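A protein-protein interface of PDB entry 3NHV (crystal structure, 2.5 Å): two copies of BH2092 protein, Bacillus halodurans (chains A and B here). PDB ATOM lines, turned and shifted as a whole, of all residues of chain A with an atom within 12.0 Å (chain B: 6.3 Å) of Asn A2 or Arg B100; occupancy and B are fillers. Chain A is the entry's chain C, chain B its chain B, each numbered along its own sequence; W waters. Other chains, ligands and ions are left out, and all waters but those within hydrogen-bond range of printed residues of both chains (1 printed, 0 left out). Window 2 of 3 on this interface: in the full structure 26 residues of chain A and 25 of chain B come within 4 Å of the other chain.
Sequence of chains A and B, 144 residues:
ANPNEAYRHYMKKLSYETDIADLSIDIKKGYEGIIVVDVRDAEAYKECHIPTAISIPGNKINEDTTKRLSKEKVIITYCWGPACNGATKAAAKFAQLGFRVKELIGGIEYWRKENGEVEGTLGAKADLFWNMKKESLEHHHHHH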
ATOM      1  N   ALA A   1      21.933  21.721  -0.852  1.00  0.00           N
ATOM      2  CA  ALA A   1      22.204  20.355  -1.400  1.00  0.00           C
ATOM      3  C   ALA A   1      21.031  19.400  -1.196  1.00  0.00           C
ATOM      4  O   ALA A   1      19.896  19.829  -0.969  1.00  0.00           O
ATOM      5  CB  ALA A   1      23.461  19.773  -0.757  1.00  0.00           C
ATOM      6  N   ASN A   2      21.314  18.103  -1.287  1.00  0.00           N
ATOM      7  CA  ASN A   2      20.282  17.085  -1.115  1.00  0.00           C
ATOM      8  C   ASN A   2      19.831  17.044   0.343  1.00  0.00           C
ATOM      9  O   ASN A   2      20.572  17.434   1.244  1.00  0.00           O
ATOM     10  CB  ASN A   2      20.810  15.706  -1.511  1.00  0.00           C
ATOM     11  CG  ASN A   2      21.194  14.865  -0.309  1.00  0.00           C
ATOM     12  OD1 ASN A   2      22.172  15.154   0.386  1.00  0.00           O
ATOM     13  ND2 ASN A   2      20.408  13.824  -0.043  1.00  0.00           N
ATOM     14  N   PRO A   3      18.608  16.555   0.591  1.00  0.00           N
ATOM     15  CA  PRO A   3      18.040  16.457   1.940  1.00  0.00           C
ATOM     16  C   PRO A   3      18.943  15.802   2.992  1.00  0.00           C
ATOM     17  O   PRO A   3      19.035  16.289   4.120  1.00  0.00           O
ATOM     18  CB  PRO A   3      16.752  15.671   1.710  1.00  0.00           C
ATOM     19  CG  PRO A   3      16.335  16.136   0.351  1.00  0.00           C
ATOM     20  CD  PRO A   3      17.640  16.089  -0.416  1.00  0.00           C
ATOM     21  N   ASN A   4      19.595  14.699   2.629  1.00  0.00           N
ATOM     22  CA  ASN A   4      20.481  13.998   3.561  1.00  0.00           C
ATOM     23  C   ASN A   4      21.560  14.928   4.110  1.00  0.00           C
ATOM     24  O   ASN A   4      21.784  14.988   5.322  1.00  0.00           O
ATOM     25  CB  ASN A   4      21.138  12.789   2.876  1.00  0.00           C
ATOM     26  CG  ASN A   4      20.172  11.615   2.698  1.00  0.00           C
ATOM     27  OD1 ASN A   4      20.464  10.665   1.963  1.00  0.00           O
ATOM     28  ND2 ASN A   4      19.023  11.672   3.377  1.00  0.00           N
ATOM     29  N   GLU A   5      22.221  15.651   3.214  1.00  0.00           N
ATOM     30  CA  GLU A   5      23.269  16.580   3.604  1.00  0.00           C
ATOM     31  C   GLU A   5      22.686  17.780   4.354  1.00  0.00           C
ATOM     32  O   GLU A   5      23.300  18.296   5.294  1.00  0.00           O
ATOM     33  CB  GLU A   5      24.036  17.052   2.365  1.00  0.00           C
ATOM     34  CG  GLU A   5      25.119  18.081   2.645  1.00  0.00           C
ATOM     35  CD  GLU A   5      25.942  18.420   1.406  1.00  0.00           C
ATOM     36  OE1 GLU A   5      26.609  17.505   0.868  1.00  0.00           O
ATOM     37  OE2 GLU A   5      25.922  19.597   0.973  1.00  0.00           O
ATOM     38  N   ALA A   6      21.496  18.211   3.946  1.00  0.00           N
ATOM     39  CA  ALA A   6      20.845  19.347   4.582  1.00  0.00           C
ATOM     40  C   ALA A   6      20.455  19.030   6.018  1.00  0.00           C
ATOM     41  O   ALA A   6      20.636  19.849   6.928  1.00  0.00           O
ATOM     42  CB  ALA A   6      19.610  19.750   3.792  1.00  0.00           C
ATOM     43  N   TYR A   7      19.904  17.838   6.216  1.00  0.00           N
ATOM     44  CA  TYR A   7      19.490  17.417   7.543  1.00  0.00           C
ATOM     45  C   TYR A   7      20.680  17.456   8.499  1.00  0.00           C
ATOM     46  O   TYR A   7      20.595  18.051   9.570  1.00  0.00           O
ATOM     47  CB  TYR A   7      18.898  16.007   7.491  1.00  0.00           C
ATOM     48  CG  TYR A   7      18.443  15.482   8.832  1.00  0.00           C
ATOM     49  CD1 TYR A   7      17.394  16.088   9.520  1.00  0.00           C
ATOM     50  CD2 TYR A   7      19.076  14.395   9.429  1.00  0.00           C
ATOM     51  CE1 TYR A   7      16.985  15.626  10.767  1.00  0.00           C
ATOM     52  CE2 TYR A   7      18.674  13.925  10.680  1.00  0.00           C
ATOM     53  CZ  TYR A   7      17.628  14.548  11.342  1.00  0.00           C
ATOM     54  OH  TYR A   7      17.227  14.107  12.580  1.00  0.00           O
ATOM     55  N   ARG A   8      21.788  16.834   8.106  1.00  0.00           N
ATOM     56  CA  ARG A   8      22.981  16.807   8.947  1.00  0.00           C
ATOM     57  C   ARG A   8      23.414  18.216   9.340  1.00  0.00           C
ATOM     58  O   ARG A   8      23.648  18.505  10.517  1.00  0.00           O
ATOM     59  CB  ARG A   8      24.131  16.081   8.231  1.00  0.00           C
ATOM     60  CG  ARG A   8      23.917  14.569   8.079  1.00  0.00           C
ATOM     61  CD  ARG A   8      25.173  13.827   7.596  1.00  0.00           C
ATOM     62  NE  ARG A   8      25.371  13.851   6.143  1.00  0.00           N
ATOM     63  CZ  ARG A   8      24.783  13.021   5.280  1.00  0.00           C
ATOM     64  NH1 ARG A   8      25.032  13.130   3.982  1.00  0.00           N
ATOM     65  NH2 ARG A   8      23.950  12.080   5.713  1.00  0.00           N
ATOM     66  N   HIS A   9      23.506  19.096   8.350  1.00  0.00           N
ATOM     67  CA  HIS A   9      23.901  20.472   8.586  1.00  0.00           C
ATOM     68  C   HIS A   9      23.051  21.143   9.664  1.00  0.00           C
ATOM     69  O   HIS A   9      23.573  21.565  10.693  1.00  0.00           O
ATOM     70  CB  HIS A   9      23.808  21.277   7.278  1.00  0.00           C
ATOM     71  CG  HIS A   9      23.882  22.759   7.480  1.00  0.00           C
ATOM     72  ND1 HIS A   9      25.033  23.400   7.886  1.00  0.00           N
ATOM     73  CD2 HIS A   9      22.926  23.714   7.404  1.00  0.00           C
ATOM     74  CE1 HIS A   9      24.782  24.686   8.053  1.00  0.00           C
ATOM     75  NE2 HIS A   9      23.511  24.904   7.768  1.00  0.00           N
ATOM     76  N   TYR A  10      21.744  21.228   9.439  1.00  0.00           N
ATOM     77  CA  TYR A  10      20.868  21.890  10.401  1.00  0.00           C
ATOM     78  C   TYR A  10      20.888  21.285  11.809  1.00  0.00           C
ATOM     79  O   TYR A  10      20.857  22.011  12.808  1.00  0.00           O
ATOM     80  CB  TYR A  10      19.439  21.933   9.866  1.00  0.00           C
ATOM     81  CG  TYR A  10      19.300  22.747   8.599  1.00  0.00           C
ATOM     82  CD1 TYR A  10      19.557  24.119   8.590  1.00  0.00           C
ATOM     83  CD2 TYR A  10      18.908  22.143   7.403  1.00  0.00           C
ATOM     84  CE1 TYR A  10      19.424  24.871   7.418  1.00  0.00           C
ATOM     85  CE2 TYR A  10      18.772  22.881   6.229  1.00  0.00           C
ATOM     86  CZ  TYR A  10      19.030  24.245   6.241  1.00  0.00           C
ATOM     87  OH  TYR A  10      18.882  24.970   5.079  1.00  0.00           O
ATOM     88  N   MET A  11      20.939  19.962  11.895  1.00  0.00           N
ATOM     89  CA  MET A  11      20.975  19.305  13.189  1.00  0.00           C
ATOM     90  C   MET A  11      22.276  19.671  13.891  1.00  0.00           C
ATOM     91  O   MET A  11      22.276  20.060  15.065  1.00  0.00           O
ATOM     92  CB  MET A  11      20.865  17.784  13.023  1.00  0.00           C
ATOM     93  CG  MET A  11      19.475  17.295  12.618  1.00  0.00           C
ATOM     94  SD  MET A  11      18.099  17.820  13.893  1.00  0.00           S
ATOM     95  CE  MET A  11      18.476  16.504  15.294  1.00  0.00           C
ATOM     96  N   TYR B  16      22.312  27.082   2.311  1.00  0.00           N
ATOM     97  CA  TYR B  16      21.325  26.721   3.332  1.00  0.00           C
ATOM     98  C   TYR B  16      20.519  27.919   3.813  1.00  0.00           C
ATOM     99  O   TYR B  16      19.762  27.813   4.778  1.00  0.00           O
ATOM    100  CB  TYR B  16      22.013  26.061   4.541  1.00  0.00           C
ATOM    101  CG  TYR B  16      22.644  24.719   4.237  1.00  0.00           C
ATOM    102  CD1 TYR B  16      21.867  23.652   3.778  1.00  0.00           C
ATOM    103  CD2 TYR B  16      24.018  24.520   4.382  1.00  0.00           C
ATOM    104  CE1 TYR B  16      22.439  22.423   3.464  1.00  0.00           C
ATOM    105  CE2 TYR B  16      24.603  23.290   4.073  1.00  0.00           C
ATOM    106  CZ  TYR B  16      23.804  22.248   3.612  1.00  0.00           C
ATOM    107  OH  TYR B  16      24.369  21.033   3.282  1.00  0.00           O
ATOM    108  N   LYS B  71       7.705  18.874  -4.230  1.00  0.00           N
ATOM    109  CA  LYS B  71       9.105  18.573  -3.938  1.00  0.00           C
ATOM    110  C   LYS B  71      10.012  19.185  -5.000  1.00  0.00           C
ATOM    111  O   LYS B  71      11.236  19.156  -4.869  1.00  0.00           O
ATOM    112  CB  LYS B  71       9.343  17.058  -3.921  1.00  0.00           C
ATOM    113  CG  LYS B  71       8.658  16.293  -2.795  1.00  0.00           C
ATOM    114  CD  LYS B  71       9.470  16.310  -1.516  1.00  0.00           C
ATOM    115  CE  LYS B  71       8.818  15.456  -0.429  1.00  0.00           C
ATOM    116  NZ  LYS B  71       8.677  14.017  -0.811  1.00  0.00           N
ATOM    117  N   LYS B  73       9.898  22.325  -5.826  1.00  0.00           N
ATOM    118  CA  LYS B  73      10.164  23.692  -5.407  1.00  0.00           C
ATOM    119  C   LYS B  73      11.131  23.720  -4.231  1.00  0.00           C
ATOM    120  O   LYS B  73      11.680  22.686  -3.845  1.00  0.00           O
ATOM    121  CB  LYS B  73       8.855  24.363  -5.020  1.00  0.00           C
ATOM    122  CG  LYS B  73       7.851  24.423  -6.152  1.00  0.00           C
ATOM    123  CD  LYS B  73       6.578  25.072  -5.684  1.00  0.00           C
ATOM    124  CE  LYS B  73       5.686  25.451  -6.843  1.00  0.00           C
ATOM    125  NZ  LYS B  73       4.485  26.163  -6.323  1.00  0.00           N
ATOM    126  N   VAL B  74      11.357  24.902  -3.667  1.00  0.00           N
ATOM    127  CA  VAL B  74      12.253  25.026  -2.518  1.00  0.00           C
ATOM    128  C   VAL B  74      11.499  25.665  -1.363  1.00  0.00           C
ATOM    129  O   VAL B  74      10.779  26.637  -1.561  1.00  0.00           O
ATOM    130  CB  VAL B  74      13.481  25.896  -2.837  1.00  0.00           C
ATOM    131  CG1 VAL B  74      14.350  26.013  -1.594  1.00  0.00           C
ATOM    132  CG2 VAL B  74      14.284  25.283  -3.982  1.00  0.00           C
ATOM    133  N   ILE B  75      11.654  25.112  -0.162  1.00  0.00           N
ATOM    134  CA  ILE B  75      10.980  25.647   1.023  1.00  0.00           C
ATOM    135  C   ILE B  75      11.861  26.684   1.736  1.00  0.00           C
ATOM    136  O   ILE B  75      13.050  26.453   1.965  1.00  0.00           O
ATOM    137  CB  ILE B  75      10.601  24.506   2.040  1.00  0.00           C
ATOM    138  CG1 ILE B  75       9.459  23.654   1.489  1.00  0.00           C
ATOM    139  CG2 ILE B  75      10.134  25.095   3.363  1.00  0.00           C
ATOM    140  CD1 ILE B  75       9.858  22.737   0.372  1.00  0.00           C
ATOM    141  N   ILE B  76      11.262  27.827   2.066  1.00  0.00           N
ATOM    142  CA  ILE B  76      11.951  28.911   2.756  1.00  0.00           C
ATOM    143  C   ILE B  76      11.244  29.099   4.091  1.00  0.00           C
ATOM    144  O   ILE B  76      10.086  29.498   4.127  1.00  0.00           O
ATOM    145  CB  ILE B  76      11.867  30.251   1.973  1.00  0.00           C
ATOM    146  CG1 ILE B  76      12.350  30.059   0.534  1.00  0.00           C
ATOM    147  CG2 ILE B  76      12.726  31.316   2.664  1.00  0.00           C
ATOM    148  CD1 ILE B  76      13.830  29.768   0.413  1.00  0.00           C
ATOM    149  N   PHE B  94      11.896  19.573   7.483  1.00  0.00           N
ATOM    150  CA  PHE B  94      11.603  19.578   6.055  1.00  0.00           C
ATOM    151  C   PHE B  94      12.627  18.746   5.297  1.00  0.00           C
ATOM    152  O   PHE B  94      12.282  18.027   4.354  1.00  0.00           O
ATOM    153  CB  PHE B  94      11.592  21.008   5.504  1.00  0.00           C
ATOM    154  CG  PHE B  94      10.254  21.685   5.594  1.00  0.00           C
ATOM    155  CD1 PHE B  94       9.215  21.316   4.740  1.00  0.00           C
ATOM    156  CD2 PHE B  94      10.036  22.696   6.526  1.00  0.00           C
ATOM    157  CE1 PHE B  94       7.977  21.950   4.813  1.00  0.00           C
ATOM    158  CE2 PHE B  94       8.807  23.336   6.610  1.00  0.00           C
ATOM    159  CZ  PHE B  94       7.769  22.965   5.750  1.00  0.00           C
ATOM    160  N   ALA B  95      13.886  18.840   5.713  1.00  0.00           N
ATOM    161  CA  ALA B  95      14.942  18.085   5.054  1.00  0.00           C
ATOM    162  C   ALA B  95      14.754  16.590   5.286  1.00  0.00           C
ATOM    163  O   ALA B  95      15.124  15.771   4.449  1.00  0.00           O
ATOM    164  CB  ALA B  95      16.307  18.528   5.566  1.00  0.00           C
ATOM    165  N   GLY B  98      12.351  14.961   2.900  1.00  0.00           N
ATOM    166  CA  GLY B  98      12.801  14.904   1.515  1.00  0.00           C
ATOM    167  C   GLY B  98      12.747  16.207   0.725  1.00  0.00           C
ATOM    168  O   GLY B  98      13.069  16.215  -0.459  1.00  0.00           O
ATOM    169  N   PHE B  99      12.344  17.302   1.370  1.00  0.00           N
ATOM    170  CA  PHE B  99      12.256  18.610   0.723  1.00  0.00           C
ATOM    171  C   PHE B  99      13.592  19.359   0.644  1.00  0.00           C
ATOM    172  O   PHE B  99      14.501  19.125   1.441  1.00  0.00           O
ATOM    173  CB  PHE B  99      11.262  19.513   1.468  1.00  0.00           C
ATOM    174  CG  PHE B  99       9.819  19.218   1.175  1.00  0.00           C
ATOM    175  CD1 PHE B  99       9.002  18.627   2.137  1.00  0.00           C
ATOM    176  CD2 PHE B  99       9.272  19.537  -0.063  1.00  0.00           C
ATOM    177  CE1 PHE B  99       7.662  18.359   1.863  1.00  0.00           C
ATOM    178  CE2 PHE B  99       7.939  19.273  -0.346  1.00  0.00           C
ATOM    179  CZ  PHE B  99       7.132  18.684   0.618  1.00  0.00           C
ATOM    180  N   ARG B 100      13.702  20.259  -0.335  1.00  0.00           N
ATOM    181  CA  ARG B 100      14.892  21.103  -0.486  1.00  0.00           C
ATOM    182  C   ARG B 100      14.463  22.340   0.304  1.00  0.00           C
ATOM    183  O   ARG B 100      13.350  22.847   0.113  1.00  0.00           O
ATOM    184  CB  ARG B 100      15.135  21.457  -1.956  1.00  0.00           C
ATOM    185  CG  ARG B 100      15.448  20.258  -2.861  1.00  0.00           C
ATOM    186  CD  ARG B 100      16.902  19.815  -2.751  1.00  0.00           C
ATOM    187  NE  ARG B 100      17.172  18.608  -3.529  1.00  0.00           N
ATOM    188  CZ  ARG B 100      18.357  18.310  -4.062  1.00  0.00           C
ATOM    189  NH1 ARG B 100      19.381  19.141  -3.904  1.00  0.00           N
ATOM    190  NH2 ARG B 100      18.523  17.184  -4.751  1.00  0.00           N
ATOM    191  N   VAL B 101      15.330  22.823   1.184  1.00  0.00           N
ATOM    192  CA  VAL B 101      14.955  23.944   2.025  1.00  0.00           C
ATOM    193  C   VAL B 101      16.102  24.872   2.398  1.00  0.00           C
ATOM    194  O   VAL B 101      17.258  24.456   2.429  1.00  0.00           O
ATOM    195  CB  VAL B 101      14.325  23.407   3.323  1.00  0.00           C
ATOM    196  CG1 VAL B 101      15.354  22.575   4.066  1.00  0.00           C
ATOM    197  CG2 VAL B 101      13.823  24.549   4.197  1.00  0.00           C
ATOM    198  N   LYS B 102      15.746  26.122   2.693  1.00  0.00           N
ATOM    199  CA  LYS B 102      16.679  27.170   3.105  1.00  0.00           C
ATOM    200  C   LYS B 102      15.962  27.977   4.189  1.00  0.00           C
ATOM    201  O   LYS B 102      14.736  28.110   4.146  1.00  0.00           O
ATOM    202  CB  LYS B 102      17.014  28.111   1.936  1.00  0.00           C
ATOM    203  CG  LYS B 102      17.714  27.464   0.750  1.00  0.00           C
ATOM    204  CD  LYS B 102      18.179  28.507  -0.266  1.00  0.00           C
ATOM    205  CE  LYS B 102      19.132  27.883  -1.288  1.00  0.00           C
ATOM    206  NZ  LYS B 102      20.033  28.887  -1.935  1.00  0.00           N
HETATM  207  O   HOH W   1      22.622  18.398  -4.371  1.00  0.00           O
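Asn A2 touches just one residue of chain B: Arg B100. Printed residues of chain B within 4 Å of Pro A3: Ala B95, Gly B98 and Phe B99. Asn A4 touches none of the printed residues of chain B. Printed residues of chain B within 4 Å of Ala A6: Tyr B16 (3.6 Å) and Ala B95 (3.9 Å). Lys B73 touches none of the printed residues of chain A. No residue of chain A comes within 4 Å of Val B74. Of chain A, only Pro A3 (3.7 Å) comes within 4 Å of Phe B99. Of chain A, only Ala A1 (3.1 Å) and Asn A2 (3.4 Å) come within 4 Å of Arg B100. Val B101 touches just one residue of chain A: Tyr A10. The nearest residue of chain B that does not touch Asn A2 is Tyr B16 (5.6 Å). The nearest residue of chain A that does not touch Arg B100 is Pro A3 (4.03 Å). The nearest printed residue of chain B that does not touch Tyr A10 is Ala B95 (4.8 Å).
The backbone NH (N) of Ile B75 sits at hydrogen-bond distance from the backbone carbonyl oxygen (O) of Arg B100, 2.8 Å away. The backbone carbonyl oxygen of Ile B75 is in hydrogen-bond range of the backbone NH of Lys B102 (2.8 Å). The backbone carbonyl oxygen of Phe B94 lies within hydrogen-bond range of the backbone NH of Phe B99 (3.1 Å). ND2 of Asn A2 sits close to N of Asn A4 (2.9 Å). OD1 of Asn A2 is in hydrogen-bond range of N of Glu A5.
No position is printed for both chains. Of the 13 pairs that touch across the chains among the printed residues, none has its exchanged pair printed and touching as well.
Water W1 bridges NH1 of Arg B100 (3.4 Å) and N of Asn A2 (3.4 Å).
Ala B95 touches Pro A3 (O to CB, 3.2 Å). Pro A3 touches Gly B98 (CG to O, 3.4 Å). Phe B99 touches Pro A3 (O to CG, 3.7 Å). Tyr B16 touches Ala A6. CB of Ala A6 touches CB of Ala B95, at 3.9 Å. Ala B95 touches Tyr A7. CD2 of His A9 touches CD2 of Tyr B16 (3.3 Å). Tyr A10 touches Lys B102.
Of the 13 printed residues of chain B, 7 touch a printed residue of chain A. Printed residues of chain B that touch a printed residue of chain A: Tyr B16, Ala B95, Gly B98, Phe B99, Arg B100, Val B101 and Lys B102. Among the printed residues, no Asp or Glu carboxylate lies within 4 Å of a Lys or Arg side-chain nitrogen of the other chain.
The side-chain hydroxyl of Tyr B16 sits close to the side-chain carboxylate of Glu A5 (3.1 Å). The backbone carbonyl oxygen of Tyr B16 lies within hydrogen-bond range of the side-chain hydroxyl of Tyr A10 (3.0 Å). The guanidinium group (NH1) of Arg B100 lies within hydrogen-bond range of the backbone carbonyl oxygen (O) of Ala A1, 3.1 Å away. The backbone carbonyl oxygen (O) of Val B101 lies within hydrogen-bond range of the side-chain hydroxyl (OH) of Tyr A10. N of Asn A2 lies close to NH1 of Arg B100 (3.4 Å).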
